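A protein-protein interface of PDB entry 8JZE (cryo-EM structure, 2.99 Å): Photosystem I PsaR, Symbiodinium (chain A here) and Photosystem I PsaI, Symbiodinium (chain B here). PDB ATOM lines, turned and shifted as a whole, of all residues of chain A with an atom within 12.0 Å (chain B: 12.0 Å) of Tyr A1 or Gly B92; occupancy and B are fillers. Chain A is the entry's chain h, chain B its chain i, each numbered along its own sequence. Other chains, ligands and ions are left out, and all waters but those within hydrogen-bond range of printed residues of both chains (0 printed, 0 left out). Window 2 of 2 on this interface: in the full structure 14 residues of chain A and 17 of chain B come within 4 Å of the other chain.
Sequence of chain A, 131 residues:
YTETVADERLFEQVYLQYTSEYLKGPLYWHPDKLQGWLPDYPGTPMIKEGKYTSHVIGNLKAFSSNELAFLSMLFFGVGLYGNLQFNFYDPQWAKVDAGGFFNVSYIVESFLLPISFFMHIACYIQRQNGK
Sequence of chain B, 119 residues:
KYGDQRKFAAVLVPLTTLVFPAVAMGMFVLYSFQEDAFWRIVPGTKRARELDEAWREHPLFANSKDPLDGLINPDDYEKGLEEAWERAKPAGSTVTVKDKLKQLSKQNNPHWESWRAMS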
ATOM      1  N   TYR A   1       3.187  16.080  35.685  1.00  0.00           N
ATOM      2  CA  TYR A   1       4.568  16.346  35.301  1.00  0.00           C
ATOM      3  C   TYR A   1       4.941  17.809  35.507  1.00  0.00           C
ATOM      4  O   TYR A   1       4.204  18.710  35.111  1.00  0.00           O
ATOM      5  CB  TYR A   1       4.805  15.953  33.840  1.00  0.00           C
ATOM      6  CG  TYR A   1       6.115  16.458  33.271  1.00  0.00           C
ATOM      7  CD1 TYR A   1       7.301  15.769  33.488  1.00  0.00           C
ATOM      8  CD2 TYR A   1       6.164  17.622  32.512  1.00  0.00           C
ATOM      9  CE1 TYR A   1       8.498  16.228  32.970  1.00  0.00           C
ATOM     10  CE2 TYR A   1       7.354  18.088  31.993  1.00  0.00           C
ATOM     11  CZ  TYR A   1       8.517  17.387  32.224  1.00  0.00           C
ATOM     12  OH  TYR A   1       9.705  17.849  31.704  1.00  0.00           O
ATOM     13  N   THR A   2       6.096  18.035  36.129  1.00  0.00           N
ATOM     14  CA  THR A   2       6.688  19.359  36.235  1.00  0.00           C
ATOM     15  C   THR A   2       8.111  19.298  35.699  1.00  0.00           C
ATOM     16  O   THR A   2       8.786  18.271  35.803  1.00  0.00           O
ATOM     17  CB  THR A   2       6.683  19.882  37.682  1.00  0.00           C
ATOM     18  OG1 THR A   2       7.265  21.192  37.719  1.00  0.00           O
ATOM     19  CG2 THR A   2       7.469  18.955  38.599  1.00  0.00           C
ATOM     20  N   GLU A   3       8.559  20.406  35.115  1.00  0.00           N
ATOM     21  CA  GLU A   3       9.842  20.432  34.416  1.00  0.00           C
ATOM     22  C   GLU A   3      10.963  20.533  35.444  1.00  0.00           C
ATOM     23  O   GLU A   3      11.317  21.617  35.909  1.00  0.00           O
ATOM     24  CB  GLU A   3       9.888  21.582  33.417  1.00  0.00           C
ATOM     25  CG  GLU A   3      11.023  21.471  32.414  1.00  0.00           C
ATOM     26  CD  GLU A   3      10.839  22.376  31.214  1.00  0.00           C
ATOM     27  OE1 GLU A   3       9.939  23.241  31.249  1.00  0.00           O
ATOM     28  OE2 GLU A   3      11.592  22.215  30.230  1.00  0.00           O
ATOM     29  N   THR A   4      11.526  19.382  35.800  1.00  0.00           N
ATOM     30  CA  THR A   4      12.678  19.358  36.686  1.00  0.00           C
ATOM     31  C   THR A   4      13.904  19.916  35.970  1.00  0.00           C
ATOM     32  O   THR A   4      13.935  20.047  34.743  1.00  0.00           O
ATOM     33  CB  THR A   4      12.962  17.937  37.173  1.00  0.00           C
ATOM     34  OG1 THR A   4      13.467  17.149  36.090  1.00  0.00           O
ATOM     35  CG2 THR A   4      11.693  17.294  37.705  1.00  0.00           C
ATOM     36  N   VAL A   5      14.925  20.254  36.759  1.00  0.00           N
ATOM     37  CA  VAL A   5      16.152  20.793  36.179  1.00  0.00           C
ATOM     38  C   VAL A   5      16.833  19.756  35.297  1.00  0.00           C
ATOM     39  O   VAL A   5      17.503  20.105  34.317  1.00  0.00           O
ATOM     40  CB  VAL A   5      17.086  21.301  37.294  1.00  0.00           C
ATOM     41  CG1 VAL A   5      16.350  22.302  38.165  1.00  0.00           C
ATOM     42  CG2 VAL A   5      17.603  20.142  38.128  1.00  0.00           C
ATOM     43  N   ALA A   6      16.670  18.471  35.620  1.00  0.00           N
ATOM     44  CA  ALA A   6      17.208  17.417  34.770  1.00  0.00           C
ATOM     45  C   ALA A   6      16.523  17.405  33.411  1.00  0.00           C
ATOM     46  O   ALA A   6      17.173  17.179  32.387  1.00  0.00           O
ATOM     47  CB  ALA A   6      17.065  16.059  35.456  1.00  0.00           C
ATOM     48  N   ASP A   7      15.210  17.639  33.382  1.00  0.00           N
ATOM     49  CA  ASP A   7      14.496  17.696  32.109  1.00  0.00           C
ATOM     50  C   ASP A   7      14.933  18.900  31.283  1.00  0.00           C
ATOM     51  O   ASP A   7      15.074  18.803  30.057  1.00  0.00           O
ATOM     52  CB  ASP A   7      12.989  17.729  32.357  1.00  0.00           C
ATOM     53  CG  ASP A   7      12.514  16.568  33.209  1.00  0.00           C
ATOM     54  OD1 ASP A   7      13.092  15.466  33.089  1.00  0.00           O
ATOM     55  OD2 ASP A   7      11.568  16.758  34.002  1.00  0.00           O
ATOM     56  N   GLU A   8      15.152  20.045  31.935  1.00  0.00           N
ATOM     57  CA  GLU A   8      15.672  21.206  31.221  1.00  0.00           C
ATOM     58  C   GLU A   8      17.056  20.919  30.653  1.00  0.00           C
ATOM     59  O   GLU A   8      17.352  21.281  29.511  1.00  0.00           O
ATOM     60  CB  GLU A   8      15.714  22.425  32.142  1.00  0.00           C
ATOM     61  CG  GLU A   8      14.352  22.921  32.600  1.00  0.00           C
ATOM     62  CD  GLU A   8      14.430  24.257  33.318  1.00  0.00           C
ATOM     63  OE1 GLU A   8      15.551  24.784  33.475  1.00  0.00           O
ATOM     64  OE2 GLU A   8      13.371  24.781  33.721  1.00  0.00           O
ATOM     65  N   ARG A   9      17.916  20.263  31.438  1.00  0.00           N
ATOM     66  CA  ARG A   9      19.241  19.890  30.949  1.00  0.00           C
ATOM     67  C   ARG A   9      19.143  18.917  29.779  1.00  0.00           C
ATOM     68  O   ARG A   9      19.928  18.993  28.826  1.00  0.00           O
ATOM     69  CB  ARG A   9      20.059  19.292  32.094  1.00  0.00           C
ATOM     70  CG  ARG A   9      21.385  18.675  31.691  1.00  0.00           C
ATOM     71  CD  ARG A   9      22.292  19.678  31.006  1.00  0.00           C
ATOM     72  NE  ARG A   9      23.597  19.101  30.711  1.00  0.00           N
ATOM     73  CZ  ARG A   9      24.701  19.363  31.394  1.00  0.00           C
ATOM     74  NH1 ARG A   9      24.703  20.225  32.396  1.00  0.00           N
ATOM     75  NH2 ARG A   9      25.833  18.752  31.058  1.00  0.00           N
ATOM     76  N   LEU A  10      18.186  17.990  29.838  1.00  0.00           N
ATOM     77  CA  LEU A  10      17.964  17.072  28.726  1.00  0.00           C
ATOM     78  C   LEU A  10      17.551  17.824  27.469  1.00  0.00           C
ATOM     79  O   LEU A  10      18.009  17.503  26.367  1.00  0.00           O
ATOM     80  CB  LEU A  10      16.905  16.038  29.104  1.00  0.00           C
ATOM     81  CG  LEU A  10      16.373  15.164  27.968  1.00  0.00           C
ATOM     82  CD1 LEU A  10      17.456  14.230  27.459  1.00  0.00           C
ATOM     83  CD2 LEU A  10      15.148  14.382  28.409  1.00  0.00           C
ATOM     84  N   PHE A  11      16.675  18.822  27.613  1.00  0.00           N
ATOM     85  CA  PHE A  11      16.310  19.631  26.454  1.00  0.00           C
ATOM     86  C   PHE A  11      17.513  20.400  25.929  1.00  0.00           C
ATOM     87  O   PHE A  11      17.673  20.555  24.715  1.00  0.00           O
ATOM     88  CB  PHE A  11      15.174  20.595  26.789  1.00  0.00           C
ATOM     89  CG  PHE A  11      14.708  21.404  25.607  1.00  0.00           C
ATOM     90  CD1 PHE A  11      13.743  20.905  24.748  1.00  0.00           C
ATOM     91  CD2 PHE A  11      15.247  22.656  25.346  1.00  0.00           C
ATOM     92  CE1 PHE A  11      13.316  21.639  23.657  1.00  0.00           C
ATOM     93  CE2 PHE A  11      14.824  23.396  24.255  1.00  0.00           C
ATOM     94  CZ  PHE A  11      13.857  22.885  23.410  1.00  0.00           C
ATOM     95  N   GLU A  12      18.358  20.905  26.830  1.00  0.00           N
ATOM     96  CA  GLU A  12      19.590  21.565  26.403  1.00  0.00           C
ATOM     97  C   GLU A  12      20.430  20.626  25.549  1.00  0.00           C
ATOM     98  O   GLU A  12      20.902  21.000  24.470  1.00  0.00           O
ATOM     99  CB  GLU A  12      20.398  22.030  27.617  1.00  0.00           C
ATOM    100  CG  GLU A  12      19.663  22.939  28.586  1.00  0.00           C
ATOM    101  CD  GLU A  12      19.768  24.401  28.223  1.00  0.00           C
ATOM    102  OE1 GLU A  12      20.804  24.800  27.655  1.00  0.00           O
ATOM    103  OE2 GLU A  12      18.811  25.151  28.509  1.00  0.00           O
ATOM    104  N   VAL A  14      19.522  17.858  23.907  1.00  0.00           N
ATOM    105  CA  VAL A  14      18.857  17.520  22.650  1.00  0.00           C
ATOM    106  C   VAL A  14      18.974  18.673  21.661  1.00  0.00           C
ATOM    107  O   VAL A  14      19.320  18.479  20.487  1.00  0.00           O
ATOM    108  CB  VAL A  14      17.386  17.147  22.906  1.00  0.00           C
ATOM    109  CG1 VAL A  14      16.610  17.119  21.601  1.00  0.00           C
ATOM    110  CG2 VAL A  14      17.296  15.803  23.601  1.00  0.00           C
ATOM    111  N   TRP B  85      13.167  16.027  19.437  1.00  0.00           N
ATOM    112  CA  TRP B  85      12.750  16.118  20.830  1.00  0.00           C
ATOM    113  C   TRP B  85      11.650  15.117  21.157  1.00  0.00           C
ATOM    114  O   TRP B  85      11.543  14.670  22.304  1.00  0.00           O
ATOM    115  CB  TRP B  85      12.291  17.540  21.147  1.00  0.00           C
ATOM    116  CG  TRP B  85      11.630  17.687  22.481  1.00  0.00           C
ATOM    117  CD1 TRP B  85      10.317  17.968  22.721  1.00  0.00           C
ATOM    118  CD2 TRP B  85      12.252  17.557  23.763  1.00  0.00           C
ATOM    119  NE1 TRP B  85      10.084  18.026  24.074  1.00  0.00           N
ATOM    120  CE2 TRP B  85      11.257  17.775  24.736  1.00  0.00           C
ATOM    121  CE3 TRP B  85      13.555  17.279  24.184  1.00  0.00           C
ATOM    122  CZ2 TRP B  85      11.524  17.723  26.101  1.00  0.00           C
ATOM    123  CZ3 TRP B  85      13.818  17.227  25.539  1.00  0.00           C
ATOM    124  CH2 TRP B  85      12.809  17.448  26.482  1.00  0.00           C
ATOM    125  N   GLU B  86      10.823  14.757  20.172  1.00  0.00           N
ATOM    126  CA  GLU B  86       9.759  13.788  20.423  1.00  0.00           C
ATOM    127  C   GLU B  86      10.324  12.426  20.806  1.00  0.00           C
ATOM    128  O   GLU B  86       9.818  11.774  21.725  1.00  0.00           O
ATOM    129  CB  GLU B  86       8.853  13.667  19.198  1.00  0.00           C
ATOM    130  CG  GLU B  86       7.839  14.790  19.066  1.00  0.00           C
ATOM    131  CD  GLU B  86       6.891  14.860  20.247  1.00  0.00           C
ATOM    132  OE1 GLU B  86       6.504  13.792  20.766  1.00  0.00           O
ATOM    133  OE2 GLU B  86       6.540  15.984  20.661  1.00  0.00           O
ATOM    134  N   ARG B  87      11.374  11.979  20.113  1.00  0.00           N
ATOM    135  CA  ARG B  87      11.979  10.689  20.422  1.00  0.00           C
ATOM    136  C   ARG B  87      12.753  10.699  21.732  1.00  0.00           C
ATOM    137  O   ARG B  87      13.063   9.624  22.255  1.00  0.00           O
ATOM    138  CB  ARG B  87      12.907  10.253  19.285  1.00  0.00           C
ATOM    139  CG  ARG B  87      14.183  11.072  19.176  1.00  0.00           C
ATOM    140  CD  ARG B  87      15.128  10.535  18.108  1.00  0.00           C
ATOM    141  NE  ARG B  87      14.584  10.662  16.762  1.00  0.00           N
ATOM    142  CZ  ARG B  87      14.002   9.676  16.092  1.00  0.00           C
ATOM    143  NH1 ARG B  87      13.867   8.470  16.616  1.00  0.00           N
ATOM    144  NH2 ARG B  87      13.548   9.907  14.863  1.00  0.00           N
ATOM    145  N   ALA B  88      13.071  11.877  22.270  1.00  0.00           N
ATOM    146  CA  ALA B  88      13.820  11.991  23.515  1.00  0.00           C
ATOM    147  C   ALA B  88      13.004  12.623  24.634  1.00  0.00           C
ATOM    148  O   ALA B  88      13.546  12.862  25.720  1.00  0.00           O
ATOM    149  CB  ALA B  88      15.106  12.792  23.290  1.00  0.00           C
ATOM    150  N   LYS B  89      11.726  12.902  24.400  1.00  0.00           N
ATOM    151  CA  LYS B  89      10.891  13.518  25.422  1.00  0.00           C
ATOM    152  C   LYS B  89      10.762  12.581  26.621  1.00  0.00           C
ATOM    153  O   LYS B  89      10.417  11.404  26.447  1.00  0.00           O
ATOM    154  CB  LYS B  89       9.512  13.849  24.851  1.00  0.00           C
ATOM    155  CG  LYS B  89       8.544  14.444  25.855  1.00  0.00           C
ATOM    156  CD  LYS B  89       7.230  14.850  25.203  1.00  0.00           C
ATOM    157  CE  LYS B  89       7.435  15.950  24.175  1.00  0.00           C
ATOM    158  NZ  LYS B  89       6.148  16.431  23.599  1.00  0.00           N
ATOM    159  N   PRO B  90      11.024  13.054  27.841  1.00  0.00           N
ATOM    160  CA  PRO B  90      11.066  12.160  29.008  1.00  0.00           C
ATOM    161  C   PRO B  90       9.675  11.771  29.484  1.00  0.00           C
ATOM    162  O   PRO B  90       8.949  12.582  30.068  1.00  0.00           O
ATOM    163  CB  PRO B  90      11.816  12.999  30.054  1.00  0.00           C
ATOM    164  CG  PRO B  90      11.505  14.406  29.688  1.00  0.00           C
ATOM    165  CD  PRO B  90      11.387  14.440  28.187  1.00  0.00           C
ATOM    166  N   ALA B  91       9.306  10.515  29.243  1.00  0.00           N
ATOM    167  CA  ALA B  91       8.078   9.895  29.764  1.00  0.00           C
ATOM    168  C   ALA B  91       6.886  10.746  29.329  1.00  0.00           C
ATOM    169  O   ALA B  91       6.791  11.090  28.140  1.00  0.00           O
ATOM    170  CB  ALA B  91       8.228   9.685  31.265  1.00  0.00           C
ATOM    171  N   GLY B  92       5.972  11.102  30.229  1.00  0.00           N
ATOM    172  CA  GLY B  92       4.818  11.902  29.868  1.00  0.00           C
ATOM    173  C   GLY B  92       5.048  13.389  30.028  1.00  0.00           C
ATOM    174  O   GLY B  92       4.215  14.096  30.603  1.00  0.00           O
ATOM    175  N   SER B  93       6.180  13.875  29.525  1.00  0.00           N
ATOM    176  CA  SER B  93       6.487  15.295  29.601  1.00  0.00           C
ATOM    177  C   SER B  93       5.519  16.098  28.738  1.00  0.00           C
ATOM    178  O   SER B  93       5.148  15.680  27.639  1.00  0.00           O
ATOM    179  CB  SER B  93       7.927  15.545  29.159  1.00  0.00           C
ATOM    180  OG  SER B  93       8.250  16.919  29.217  1.00  0.00           O
ATOM    181  N   THR B  94       5.108  17.258  29.248  1.00  0.00           N
ATOM    182  CA  THR B  94       4.101  18.084  28.596  1.00  0.00           C
ATOM    183  C   THR B  94       4.684  19.319  27.916  1.00  0.00           C
ATOM    184  O   THR B  94       3.921  20.191  27.488  1.00  0.00           O
ATOM    185  CB  THR B  94       3.033  18.510  29.606  1.00  0.00           C
ATOM    186  OG1 THR B  94       2.037  19.301  28.945  1.00  0.00           O
ATOM    187  CG2 THR B  94       3.656  19.327  30.725  1.00  0.00           C
ATOM    188  N   VAL B  95       6.004  19.416  27.800  1.00  0.00           N
ATOM    189  CA  VAL B  95       6.636  20.566  27.165  1.00  0.00           C
ATOM    190  C   VAL B  95       6.837  20.269  25.685  1.00  0.00           C
ATOM    191  O   VAL B  95       7.360  19.211  25.315  1.00  0.00           O
ATOM    192  CB  VAL B  95       7.969  20.918  27.851  1.00  0.00           C
ATOM    193  CG1 VAL B  95       8.863  19.698  27.972  1.00  0.00           C
ATOM    194  CG2 VAL B  95       8.683  22.021  27.090  1.00  0.00           C
ATOM    195  N   THR B  96       6.397  21.191  24.838  1.00  0.00           N
ATOM    196  CA  THR B  96       6.628  21.115  23.404  1.00  0.00           C
ATOM    197  C   THR B  96       7.848  21.952  23.040  1.00  0.00           C
ATOM    198  O   THR B  96       8.361  22.729  23.844  1.00  0.00           O
ATOM    199  CB  THR B  96       5.396  21.592  22.628  1.00  0.00           C
ATOM    200  OG1 THR B  96       5.273  23.014  22.747  1.00  0.00           O
ATOM    201  CG2 THR B  96       4.137  20.938  23.174  1.00  0.00           C
ATOM    202  N   VAL B  97       8.328  21.770  21.810  1.00  0.00           N
ATOM    203  CA  VAL B  97       9.478  22.542  21.352  1.00  0.00           C
ATOM    204  C   VAL B  97       9.098  24.001  21.143  1.00  0.00           C
ATOM    205  O   VAL B  97       9.873  24.912  21.465  1.00  0.00           O
ATOM    206  CB  VAL B  97      10.065  21.919  20.074  1.00  0.00           C
ATOM    207  CG1 VAL B  97      11.100  22.840  19.457  1.00  0.00           C
ATOM    208  CG2 VAL B  97      10.682  20.583  20.396  1.00  0.00           C
ATOM    209  N   ASP B  99       6.715  26.128  22.479  1.00  0.00           N
ATOM    210  CA  ASP B  99       6.601  26.988  23.651  1.00  0.00           C
ATOM    211  C   ASP B  99       7.886  26.993  24.467  1.00  0.00           C
ATOM    212  O   ASP B  99       8.186  27.987  25.136  1.00  0.00           O
ATOM    213  CB  ASP B  99       5.409  26.570  24.517  1.00  0.00           C
ATOM    214  CG  ASP B  99       5.473  25.122  24.951  1.00  0.00           C
ATOM    215  OD1 ASP B  99       6.317  24.376  24.419  1.00  0.00           O
ATOM    216  OD2 ASP B  99       4.673  24.727  25.826  1.00  0.00           O
ATOM    217  N   LYS B 100       8.666  25.910  24.412  1.00  0.00           N
ATOM    218  CA  LYS B 100       9.962  25.904  25.083  1.00  0.00           C
ATOM    219  C   LYS B 100      10.888  26.955  24.485  1.00  0.00           C
ATOM    220  O   LYS B 100      11.511  27.736  25.213  1.00  0.00           O
ATOM    221  CB  LYS B 100      10.595  24.516  24.998  1.00  0.00           C
ATOM    222  CG  LYS B 100      11.837  24.351  25.851  1.00  0.00           C
ATOM    223  CD  LYS B 100      11.541  24.631  27.312  1.00  0.00           C
ATOM    224  CE  LYS B 100      12.774  24.429  28.176  1.00  0.00           C
ATOM    225  NZ  LYS B 100      12.470  24.644  29.616  1.00  0.00           N
ATOM    226  N   GLN B 103       9.555  30.515  25.381  1.00  0.00           N
ATOM    227  CA  GLN B 103       9.874  30.958  26.732  1.00  0.00           C
ATOM    228  C   GLN B 103      11.374  31.051  26.981  1.00  0.00           C
ATOM    229  O   GLN B 103      11.789  31.737  27.921  1.00  0.00           O
ATOM    230  CB  GLN B 103       9.226  30.030  27.762  1.00  0.00           C
ATOM    231  CG  GLN B 103       9.912  28.685  27.942  1.00  0.00           C
ATOM    232  CD  GLN B 103      10.759  28.630  29.200  1.00  0.00           C
ATOM    233  OE1 GLN B 103      11.030  29.656  29.821  1.00  0.00           O
ATOM    234  NE2 GLN B 103      11.176  27.429  29.583  1.00  0.00           N
ATOM    235  N   LEU B 104      12.195  30.380  26.169  1.00  0.00           N
ATOM    236  CA  LEU B 104      13.638  30.556  26.256  1.00  0.00           C
ATOM    237  C   LEU B 104      14.115  31.801  25.524  1.00  0.00           C
ATOM    238  O   LEU B 104      15.228  32.266  25.781  1.00  0.00           O
ATOM    239  CB  LEU B 104      14.358  29.323  25.704  1.00  0.00           C
ATOM    240  CG  LEU B 104      14.441  28.125  26.652  1.00  0.00           C
ATOM    241  CD1 LEU B 104      14.955  26.888  25.939  1.00  0.00           C
ATOM    242  CD2 LEU B 104      15.326  28.457  27.839  1.00  0.00           C
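The indole nitrogen of Trp B85 sits at hydrogen-bond distance from the backbone carbonyl oxygen of Val B95. The side-chain carboxylate of Asp A7 is in hydrogen-bond range of the side-chain hydroxyl of Tyr A1 (3.2 Å). NZ of Lys B100 lies close to NE2 of Gln B103, 3.1 Å away. OG1 of Thr A4 lies within hydrogen-bond range of OD2 of Asp A7 (2.8 Å).
Among the printed residues, pairs that only touch across the chains: Tyr A1 with Gly B92 (3.8 Å), Tyr A1 with Thr B94 (3.4 Å), Asp A7 with Pro B90 (3.9 Å), Glu A8 with Lys B100 (3.9 Å), Leu A10 with Ala B88 (3.5 Å), Leu A10 with Pro B90 (3.8 Å), Phe A11 with Trp B85 (3.6 Å), Phe A11 with Lys B100 (3.5 Å), Phe A11 with Leu B104 (3.9 Å) and Val A14 with Ala B88 (3.7 Å).
OH of Tyr A1 sits at hydrogen-bond distance from OG of Ser B93 (3.0 Å). The side-chain carboxylate (OE2) of Glu A3 lies within salt-bridge range of the side-chain amino group (NZ) of Lys B100 (2.7 Å).
Of chain B, only Gly B92 (3.8 Å), Ser B93 (3.0 Å) and Thr B94 (3.4 Å) come within 4 Å of Tyr A1. Gly B92 touches just one residue of chain A: Tyr A1 (3.8 Å). Of the printed residues of chain B, Glu A3 touches Lys B100. No residue of chain B comes within 4 Å of Thr A4. Asp A7 touches just one residue of chain B: Pro B90 (3.9 Å). No residue of chain A comes within 4 Å of Ala B91. No residue of chain A comes within 4 Å of Val B95. Of the printed residues of chain B, Phe A11 touches Trp B85 (3.6 Å), Lys B100 (3.5 Å) and Leu B104 (3.9 Å). Of the printed residues of chain A, Ala B88 touches Leu A10 and Val A14. Printed residues of chain A within 4 Å of Leu B104: Phe A11 (3.9 Å). Of the printed residues of chain A, Trp B85 touches Phe A11. Printed residues of chain B within 4 Å of Leu A10: Ala B88 and Pro B90. Glu A12 touches none of the printed residues of chain B. Glu B86 touches none of the printed residues of chain A. The nearest residue of chain A that does not touch Gly B92 is Thr A2 (7.0 Å). The nearest printed residue of chain B that does not touch Glu A8 is Gln B103 (5.4 Å).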
